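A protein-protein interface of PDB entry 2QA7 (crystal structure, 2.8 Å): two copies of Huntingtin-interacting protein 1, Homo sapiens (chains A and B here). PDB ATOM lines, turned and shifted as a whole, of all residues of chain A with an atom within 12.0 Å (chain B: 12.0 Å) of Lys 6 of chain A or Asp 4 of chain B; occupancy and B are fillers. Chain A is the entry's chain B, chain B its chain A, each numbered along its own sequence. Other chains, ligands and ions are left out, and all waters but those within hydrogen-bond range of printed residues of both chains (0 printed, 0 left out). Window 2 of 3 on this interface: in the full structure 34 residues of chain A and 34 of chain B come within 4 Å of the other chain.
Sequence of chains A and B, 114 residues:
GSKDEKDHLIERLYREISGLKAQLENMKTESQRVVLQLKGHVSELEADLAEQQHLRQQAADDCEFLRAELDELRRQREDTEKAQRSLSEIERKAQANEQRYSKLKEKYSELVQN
Hydrophobic or aromatic side chains of chain B within 4 Å of the printed part of chain A: Leu 9, Ile 10, Leu 13, Tyr 14 and Ile 17.
Of the 12 printed residues of chain A, 6 touch a printed residue of chain B.
Printed residues of chain A that touch a printed residue of chain B: Lys 6, Asp 7, Leu 9, Ile 10, Leu 13 and Tyr 14.
Hydrophobic or aromatic side chains of chain A that line the printed part of chain B: Leu 9, Ile 10, Leu 13 and Tyr 14.
Among the printed residues, 11 pairs touch across the chains.
Among the printed residues, Asp or Glu carboxylates within 4 Å of a Lys or Arg side-chain nitrogen of the other chain: Lys 6 of chain A with Asp 7 of chain B (3.0 Å) and Asp 7 of chain A with Lys 6 of chain B (3.1 Å).
Among the printed residues, merely in contact across the chains: Lys 6 of chain A with Asp 4 of chain B (3.7 Å), Leu 9 of chain A with Tyr 14 of chain B (3.6 Å), Ile 10 of chain A with Ile 10 of chain B (3.6 Å), Ile 10 of chain A with Leu 13 of chain B (3.9 Å), Leu 13 of chain A with Leu 13 of chain B (3.9 Å), Leu 13 of chain A with Tyr 14 of chain B (3.4 Å), Leu 13 of chain A with Ile 17 of chain B (3.8 Å), Tyr 14 of chain A with Leu 9 of chain B (3.6 Å) and Tyr 14 of chain A with Leu 13 of chain B (3.4 Å).
Lys 6 of chain A touches Asp 4 of chain B, but with the chains exchanged Asp 4 of chain A does not touch Lys 6 of chain B (6.5 Å).
Lys 6 of chain A touches Asp 7 of chain B, and with the chains exchanged Asp 7 of chain A touches Lys 6 of chain B.
Ile 10 of chain A touches its own counterpart, Ile 10 of chain B.
Ile 10 of chain A touches Leu 13 of chain B, but with the chains exchanged Leu 13 of chain A does not touch Ile 10 of chain B (4.3 Å).
No residue of chain B comes within 4 Å of Glu 5 of chain A.
Lys 6 of chain A touches just these residues of chain B: Asp 4 (3.7 Å) and Asp 7 (3.0 Å).
Of chain B, only Lys 6 comes within 4 Å of Asp 7 of chain A.
Of chain B, only Tyr 14 (3.6 Å) comes within 4 Å of Leu 9 of chain A.
Ile 10 of chain A touches two residues of chain B.
Of the printed residues of chain B, Tyr 14 of chain A touches Leu 9 and Leu 13.
Of chain A, only Lys 6 comes within 4 Å of Asp 4 of chain B.
No residue of chain A comes within 4 Å of Glu 5 of chain B.
Of chain A, only Asp 7 comes within 4 Å of Lys 6 of chain B.
Asp 7 of chain B touches just one residue of chain A: Lys 6 (3.0 Å).
No residue of chain A comes within 4 Å of His 8 of chain B.
Of the printed residues of chain A, Leu 9 of chain B touches Tyr 14.
Of the printed residues of chain A, Ile 10 of chain B touches Ile 10.
Glu 11 of chain B touches none of the printed residues of chain A.
Of the printed residues of chain A, Leu 13 of chain B touches Ile 10 (3.9 Å), Leu 13 (3.9 Å) and Tyr 14 (3.4 Å).
The nearest residue of chain B that does not touch Lys 6 of chain A is Ile 10 of chain B (4.2 Å).
The nearest printed residue of chain A that does not touch Ile 17 of chain B is Tyr 14 of chain A (5.8 Å).
The side-chain carboxylate of Asp 7 of chain A is in salt-bridge range of the side-chain amino group of Lys 6 of chain B (3.1 Å).
OD1 of Asp 7 of chain B lies within salt-bridge range of NZ of Lys 6 of chain A, 3.0 Å away.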
ATOM      1  N   ASP A   4      16.559   9.931  -5.267  1.00  0.00           N
ATOM      2  CA  ASP A   4      16.313   8.482  -5.539  1.00  0.00           C
ATOM      3  C   ASP A   4      16.804   7.622  -4.369  1.00  0.00           C
ATOM      4  O   ASP A   4      17.680   8.056  -3.615  1.00  0.00           O
ATOM      5  CB  ASP A   4      17.029   8.069  -6.831  1.00  0.00           C
ATOM      6  CG  ASP A   4      16.568   8.864  -8.022  1.00  0.00           C
ATOM      7  OD1 ASP A   4      15.392   8.799  -8.432  1.00  0.00           O
ATOM      8  OD2 ASP A   4      17.398   9.591  -8.552  1.00  0.00           O
ATOM      9  N   GLU A   5      16.227   6.420  -4.234  1.00  0.00           N
ATOM     10  CA  GLU A   5      16.556   5.438  -3.183  1.00  0.00           C
ATOM     11  C   GLU A   5      15.273   4.758  -2.706  1.00  0.00           C
ATOM     12  O   GLU A   5      14.666   3.963  -3.419  1.00  0.00           O
ATOM     13  CB  GLU A   5      17.210   6.112  -1.980  1.00  0.00           C
ATOM     14  CG  GLU A   5      16.373   7.247  -1.409  1.00  0.00           C
ATOM     15  CD  GLU A   5      16.864   7.701  -0.074  1.00  0.00           C
ATOM     16  OE1 GLU A   5      16.781   6.916   0.897  1.00  0.00           O
ATOM     17  OE2 GLU A   5      17.337   8.847  -0.002  1.00  0.00           O
ATOM     18  N   LYS A   6      14.885   5.069  -1.475  1.00  0.00           N
ATOM     19  CA  LYS A   6      13.666   4.560  -0.888  1.00  0.00           C
ATOM     20  C   LYS A   6      12.552   5.229  -1.671  1.00  0.00           C
ATOM     21  O   LYS A   6      11.443   4.705  -1.778  1.00  0.00           O
ATOM     22  CB  LYS A   6      13.551   4.999   0.558  1.00  0.00           C
ATOM     23  CG  LYS A   6      14.503   4.355   1.547  1.00  0.00           C
ATOM     24  CD  LYS A   6      14.216   4.986   2.901  1.00  0.00           C
ATOM     25  CE  LYS A   6      15.037   4.415   4.016  1.00  0.00           C
ATOM     26  NZ  LYS A   6      14.739   5.191   5.256  1.00  0.00           N
ATOM     27  N   ASP A   7      12.851   6.406  -2.209  1.00  0.00           N
ATOM     28  CA  ASP A   7      11.877   7.141  -2.992  1.00  0.00           C
ATOM     29  C   ASP A   7      11.361   6.274  -4.114  1.00  0.00           C
ATOM     30  O   ASP A   7      10.183   6.321  -4.453  1.00  0.00           O
ATOM     31  CB  ASP A   7      12.497   8.402  -3.559  1.00  0.00           C
ATOM     32  CG  ASP A   7      12.701   9.451  -2.508  1.00  0.00           C
ATOM     33  OD1 ASP A   7      11.692  10.008  -2.022  1.00  0.00           O
ATOM     34  OD2 ASP A   7      13.868   9.704  -2.158  1.00  0.00           O
ATOM     35  N   HIS A   8      12.242   5.476  -4.693  1.00  0.00           N
ATOM     36  CA  HIS A   8      11.835   4.579  -5.759  1.00  0.00           C
ATOM     37  C   HIS A   8      10.906   3.497  -5.198  1.00  0.00           C
ATOM     38  O   HIS A   8       9.866   3.196  -5.790  1.00  0.00           O
ATOM     39  CB  HIS A   8      13.070   3.956  -6.402  1.00  0.00           C
ATOM     40  CG  HIS A   8      13.944   4.947  -7.105  1.00  0.00           C
ATOM     41  ND1 HIS A   8      15.281   4.721  -7.342  1.00  0.00           N
ATOM     42  CD2 HIS A   8      13.668   6.163  -7.635  1.00  0.00           C
ATOM     43  CE1 HIS A   8      15.793   5.753  -7.987  1.00  0.00           C
ATOM     44  NE2 HIS A   8      14.835   6.643  -8.176  1.00  0.00           N
ATOM     45  N   LEU A   9      11.264   2.927  -4.049  1.00  0.00           N
ATOM     46  CA  LEU A   9      10.430   1.896  -3.438  1.00  0.00           C
ATOM     47  C   LEU A   9       9.046   2.490  -3.286  1.00  0.00           C
ATOM     48  O   LEU A   9       8.036   1.832  -3.570  1.00  0.00           O
ATOM     49  CB  LEU A   9      10.943   1.500  -2.054  1.00  0.00           C
ATOM     50  CG  LEU A   9      10.788   0.016  -1.675  1.00  0.00           C
ATOM     51  CD1 LEU A   9      10.907  -0.107  -0.163  1.00  0.00           C
ATOM     52  CD2 LEU A   9       9.452  -0.552  -2.133  1.00  0.00           C
ATOM     53  N   ILE A  10       9.010   3.744  -2.839  1.00  0.00           N
ATOM     54  CA  ILE A  10       7.747   4.434  -2.663  1.00  0.00           C
ATOM     55  C   ILE A  10       6.988   4.490  -3.998  1.00  0.00           C
ATOM     56  O   ILE A  10       5.887   3.940  -4.108  1.00  0.00           O
ATOM     57  CB  ILE A  10       7.953   5.858  -2.139  1.00  0.00           C
ATOM     58  CG1 ILE A  10       8.954   5.859  -0.973  1.00  0.00           C
ATOM     59  CG2 ILE A  10       6.617   6.440  -1.724  1.00  0.00           C
ATOM     60  CD1 ILE A  10       8.371   6.005   0.420  1.00  0.00           C
ATOM     61  N   GLU A  11       7.572   5.121  -5.017  1.00  0.00           N
ATOM     62  CA  GLU A  11       6.899   5.226  -6.316  1.00  0.00           C
ATOM     63  C   GLU A  11       6.472   3.855  -6.822  1.00  0.00           C
ATOM     64  O   GLU A  11       5.369   3.677  -7.357  1.00  0.00           O
ATOM     65  CB  GLU A  11       7.810   5.904  -7.355  1.00  0.00           C
ATOM     66  CG  GLU A  11       9.113   5.157  -7.667  1.00  0.00           C
ATOM     67  CD  GLU A  11      10.049   5.928  -8.611  1.00  0.00           C
ATOM     68  OE1 GLU A  11      10.204   7.157  -8.430  1.00  0.00           O
ATOM     69  OE2 GLU A  11      10.646   5.300  -9.519  1.00  0.00           O
ATOM     70  N   ARG A  12       7.348   2.879  -6.636  1.00  0.00           N
ATOM     71  CA  ARG A  12       7.061   1.528  -7.068  1.00  0.00           C
ATOM     72  C   ARG A  12       5.781   1.035  -6.376  1.00  0.00           C
ATOM     73  O   ARG A  12       4.846   0.571  -7.033  1.00  0.00           O
ATOM     74  CB  ARG A  12       8.260   0.637  -6.739  1.00  0.00           C
ATOM     75  CG  ARG A  12       8.402  -0.599  -7.607  1.00  0.00           C
ATOM     76  CD  ARG A  12       7.309  -1.582  -7.292  1.00  0.00           C
ATOM     77  NE  ARG A  12       7.468  -2.849  -7.992  1.00  0.00           N
ATOM     78  CZ  ARG A  12       6.794  -3.947  -7.672  1.00  0.00           C
ATOM     79  NH1 ARG A  12       5.928  -3.915  -6.662  1.00  0.00           N
ATOM     80  NH2 ARG A  12       6.974  -5.068  -8.359  1.00  0.00           N
ATOM     81  N   LEU A  13       5.729   1.162  -5.055  1.00  0.00           N
ATOM     82  CA  LEU A  13       4.560   0.730  -4.307  1.00  0.00           C
ATOM     83  C   LEU A  13       3.304   1.516  -4.703  1.00  0.00           C
ATOM     84  O   LEU A  13       2.228   0.942  -4.823  1.00  0.00           O
ATOM     85  CB  LEU A  13       4.812   0.864  -2.812  1.00  0.00           C
ATOM     86  CG  LEU A  13       5.967   0.039  -2.249  1.00  0.00           C
ATOM     87  CD1 LEU A  13       6.206   0.423  -0.808  1.00  0.00           C
ATOM     88  CD2 LEU A  13       5.652  -1.439  -2.354  1.00  0.00           C
ATOM     89  N   TYR A  14       3.416   2.823  -4.901  1.00  0.00           N
ATOM     90  CA  TYR A  14       2.238   3.583  -5.308  1.00  0.00           C
ATOM     91  C   TYR A  14       1.723   3.034  -6.629  1.00  0.00           C
ATOM     92  O   TYR A  14       0.513   2.911  -6.829  1.00  0.00           O
ATOM     93  CB  TYR A  14       2.554   5.077  -5.478  1.00  0.00           C
ATOM     94  CG  TYR A  14       2.427   5.882  -4.206  1.00  0.00           C
ATOM     95  CD1 TYR A  14       3.352   6.886  -3.890  1.00  0.00           C
ATOM     96  CD2 TYR A  14       1.418   5.602  -3.290  1.00  0.00           C
ATOM     97  CE1 TYR A  14       3.276   7.579  -2.683  1.00  0.00           C
ATOM     98  CE2 TYR A  14       1.330   6.281  -2.090  1.00  0.00           C
ATOM     99  CZ  TYR A  14       2.259   7.266  -1.782  1.00  0.00           C
ATOM    100  OH  TYR A  14       2.173   7.898  -0.558  1.00  0.00           O
ATOM    101  N   ARG A  15       2.642   2.701  -7.531  1.00  0.00           N
ATOM    102  CA  ARG A  15       2.249   2.177  -8.832  1.00  0.00           C
ATOM    103  C   ARG A  15       1.436   0.889  -8.663  1.00  0.00           C
ATOM    104  O   ARG A  15       0.381   0.711  -9.294  1.00  0.00           O
ATOM    105  CB  ARG A  15       3.492   1.914  -9.690  1.00  0.00           C
ATOM    106  CG  ARG A  15       3.189   1.446 -11.112  1.00  0.00           C
ATOM    107  CD  ARG A  15       4.452   1.156 -11.902  1.00  0.00           C
ATOM    108  NE  ARG A  15       4.169   0.575 -13.215  1.00  0.00           N
ATOM    109  CZ  ARG A  15       5.101   0.212 -14.098  1.00  0.00           C
ATOM    110  NH1 ARG A  15       6.388   0.366 -13.817  1.00  0.00           N
ATOM    111  NH2 ARG A  15       4.749  -0.313 -15.266  1.00  0.00           N
ATOM    112  N   ASP B   4      13.748   7.875   7.526  1.00  0.00           N
ATOM    113  CA  ASP B   4      12.860   7.224   8.540  1.00  0.00           C
ATOM    114  C   ASP B   4      11.391   7.605   8.412  1.00  0.00           C
ATOM    115  O   ASP B   4      10.533   6.733   8.387  1.00  0.00           O
ATOM    116  CB  ASP B   4      13.331   7.530   9.967  1.00  0.00           C
ATOM    117  CG  ASP B   4      12.400   6.946  11.032  1.00  0.00           C
ATOM    118  OD1 ASP B   4      11.305   7.514  11.248  1.00  0.00           O
ATOM    119  OD2 ASP B   4      12.761   5.915  11.647  1.00  0.00           O
ATOM    120  N   GLU B   5      11.089   8.897   8.352  1.00  0.00           N
ATOM    121  CA  GLU B   5       9.700   9.327   8.207  1.00  0.00           C
ATOM    122  C   GLU B   5       9.122   8.598   7.007  1.00  0.00           C
ATOM    123  O   GLU B   5       7.930   8.314   6.943  1.00  0.00           O
ATOM    124  CB  GLU B   5       9.622  10.837   7.981  1.00  0.00           C
ATOM    125  CG  GLU B   5      10.153  11.652   9.151  1.00  0.00           C
ATOM    126  CD  GLU B   5      10.168  13.146   8.883  1.00  0.00           C
ATOM    127  OE1 GLU B   5       9.129  13.686   8.439  1.00  0.00           O
ATOM    128  OE2 GLU B   5      11.221  13.775   9.128  1.00  0.00           O
ATOM    129  N   LYS B   6       9.987   8.279   6.055  1.00  0.00           N
ATOM    130  CA  LYS B   6       9.563   7.575   4.867  1.00  0.00           C
ATOM    131  C   LYS B   6       9.346   6.097   5.168  1.00  0.00           C
ATOM    132  O   LYS B   6       8.605   5.410   4.461  1.00  0.00           O
ATOM    133  CB  LYS B   6      10.587   7.797   3.756  1.00  0.00           C
ATOM    134  CG  LYS B   6      10.593   9.255   3.309  1.00  0.00           C
ATOM    135  CD  LYS B   6      11.308   9.494   1.998  1.00  0.00           C
ATOM    136  CE  LYS B   6      12.801   9.360   2.142  1.00  0.00           C
ATOM    137  NZ  LYS B   6      13.443   9.862   0.906  1.00  0.00           N
ATOM    138  N   ASP B   7       9.980   5.613   6.232  1.00  0.00           N
ATOM    139  CA  ASP B   7       9.803   4.226   6.640  1.00  0.00           C
ATOM    140  C   ASP B   7       8.337   4.047   7.011  1.00  0.00           C
ATOM    141  O   ASP B   7       7.720   3.052   6.653  1.00  0.00           O
ATOM    142  CB  ASP B   7      10.672   3.879   7.853  1.00  0.00           C
ATOM    143  CG  ASP B   7      12.157   3.946   7.554  1.00  0.00           C
ATOM    144  OD1 ASP B   7      12.576   3.512   6.460  1.00  0.00           O
ATOM    145  OD2 ASP B   7      12.917   4.419   8.423  1.00  0.00           O
ATOM    146  N   HIS B   8       7.781   5.015   7.734  1.00  0.00           N
ATOM    147  CA  HIS B   8       6.379   4.952   8.132  1.00  0.00           C
ATOM    148  C   HIS B   8       5.513   4.836   6.891  1.00  0.00           C
ATOM    149  O   HIS B   8       4.667   3.950   6.806  1.00  0.00           O
ATOM    150  CB  HIS B   8       5.969   6.201   8.931  1.00  0.00           C
ATOM    151  CG  HIS B   8       6.548   6.254  10.309  1.00  0.00           C
ATOM    152  ND1 HIS B   8       6.624   5.147  11.126  1.00  0.00           N
ATOM    153  CD2 HIS B   8       7.096   7.275  11.010  1.00  0.00           C
ATOM    154  CE1 HIS B   8       7.199   5.482  12.267  1.00  0.00           C
ATOM    155  NE2 HIS B   8       7.495   6.768  12.224  1.00  0.00           N
ATOM    156  N   LEU B   9       5.738   5.727   5.929  1.00  0.00           N
ATOM    157  CA  LEU B   9       4.971   5.703   4.699  1.00  0.00           C
ATOM    158  C   LEU B   9       5.133   4.375   3.977  1.00  0.00           C
ATOM    159  O   LEU B   9       4.162   3.844   3.437  1.00  0.00           O
ATOM    160  CB  LEU B   9       5.382   6.849   3.768  1.00  0.00           C
ATOM    161  CG  LEU B   9       4.637   6.854   2.422  1.00  0.00           C
ATOM    162  CD1 LEU B   9       3.141   6.773   2.675  1.00  0.00           C
ATOM    163  CD2 LEU B   9       4.979   8.105   1.613  1.00  0.00           C
ATOM    164  N   ILE B  10       6.354   3.839   3.961  1.00  0.00           N
ATOM    165  CA  ILE B  10       6.601   2.550   3.306  1.00  0.00           C
ATOM    166  C   ILE B  10       5.759   1.465   3.984  1.00  0.00           C
ATOM    167  O   ILE B  10       5.089   0.681   3.312  1.00  0.00           O
ATOM    168  CB  ILE B  10       8.115   2.166   3.345  1.00  0.00           C
ATOM    169  CG1 ILE B  10       8.889   3.012   2.329  1.00  0.00           C
ATOM    170  CG2 ILE B  10       8.310   0.692   3.017  1.00  0.00           C
ATOM    171  CD1 ILE B  10      10.390   2.910   2.458  1.00  0.00           C
ATOM    172  N   GLU B  11       5.781   1.432   5.312  1.00  0.00           N
ATOM    173  CA  GLU B  11       5.001   0.461   6.070  1.00  0.00           C
ATOM    174  C   GLU B  11       3.517   0.575   5.725  1.00  0.00           C
ATOM    175  O   GLU B  11       2.828  -0.420   5.534  1.00  0.00           O
ATOM    176  CB  GLU B  11       5.178   0.693   7.565  1.00  0.00           C
ATOM    177  CG  GLU B  11       6.495   0.218   8.133  1.00  0.00           C
ATOM    178  CD  GLU B  11       6.778   0.852   9.478  1.00  0.00           C
ATOM    179  OE1 GLU B  11       5.822   0.994  10.279  1.00  0.00           O
ATOM    180  OE2 GLU B  11       7.950   1.207   9.734  1.00  0.00           O
ATOM    181  N   ARG B  12       3.016   1.796   5.657  1.00  0.00           N
ATOM    182  CA  ARG B  12       1.618   1.976   5.337  1.00  0.00           C
ATOM    183  C   ARG B  12       1.316   1.415   3.944  1.00  0.00           C
ATOM    184  O   ARG B  12       0.368   0.666   3.755  1.00  0.00           O
ATOM    185  CB  ARG B  12       1.258   3.460   5.397  1.00  0.00           C
ATOM    186  CG  ARG B  12      -0.188   3.768   5.061  1.00  0.00           C
ATOM    187  CD  ARG B  12      -0.370   5.232   4.835  1.00  0.00           C
ATOM    188  NE  ARG B  12      -0.247   5.983   6.081  1.00  0.00           N
ATOM    189  CZ  ARG B  12      -0.241   7.310   6.152  1.00  0.00           C
ATOM    190  NH1 ARG B  12      -0.335   8.032   5.044  1.00  0.00           N
ATOM    191  NH2 ARG B  12      -0.194   7.913   7.330  1.00  0.00           N
ATOM    192  N   LEU B  13       2.129   1.772   2.965  1.00  0.00           N
ATOM    193  CA  LEU B  13       1.902   1.296   1.619  1.00  0.00           C
ATOM    194  C   LEU B  13       1.884  -0.228   1.525  1.00  0.00           C
ATOM    195  O   LEU B  13       1.035  -0.803   0.843  1.00  0.00           O
ATOM    196  CB  LEU B  13       2.952   1.896   0.681  1.00  0.00           C
ATOM    197  CG  LEU B  13       2.949   3.431   0.656  1.00  0.00           C
ATOM    198  CD1 LEU B  13       3.865   3.910  -0.449  1.00  0.00           C
ATOM    199  CD2 LEU B  13       1.538   3.954   0.427  1.00  0.00           C
ATOM    200  N   TYR B  14       2.805  -0.897   2.203  1.00  0.00           N
ATOM    201  CA  TYR B  14       2.808  -2.356   2.149  1.00  0.00           C
ATOM    202  C   TYR B  14       1.515  -2.941   2.725  1.00  0.00           C
ATOM    203  O   TYR B  14       1.066  -4.014   2.319  1.00  0.00           O
ATOM    204  CB  TYR B  14       4.015  -2.922   2.898  1.00  0.00           C
ATOM    205  CG  TYR B  14       5.224  -3.125   2.015  1.00  0.00           C
ATOM    206  CD1 TYR B  14       6.481  -2.670   2.402  1.00  0.00           C
ATOM    207  CD2 TYR B  14       5.112  -3.759   0.787  1.00  0.00           C
ATOM    208  CE1 TYR B  14       7.589  -2.842   1.585  1.00  0.00           C
ATOM    209  CE2 TYR B  14       6.217  -3.932  -0.038  1.00  0.00           C
ATOM    210  CZ  TYR B  14       7.447  -3.470   0.370  1.00  0.00           C
ATOM    211  OH  TYR B  14       8.533  -3.625  -0.447  1.00  0.00           O
ATOM    212  N   ILE B  17      -1.403  -2.394   0.193  1.00  0.00           N
ATOM    213  CA  ILE B  17      -1.304  -3.430  -0.819  1.00  0.00           C
ATOM    214  C   ILE B  17      -1.837  -4.776  -0.339  1.00  0.00           C
ATOM    215  O   ILE B  17      -2.721  -5.349  -0.983  1.00  0.00           O
ATOM    216  CB  ILE B  17       0.163  -3.570  -1.314  1.00  0.00           C
ATOM    217  CG1 ILE B  17       0.522  -2.344  -2.154  1.00  0.00           C
ATOM    218  CG2 ILE B  17       0.337  -4.828  -2.140  1.00  0.00           C
ATOM    219  CD1 ILE B  17       1.967  -2.243  -2.500  1.00  0.00           C
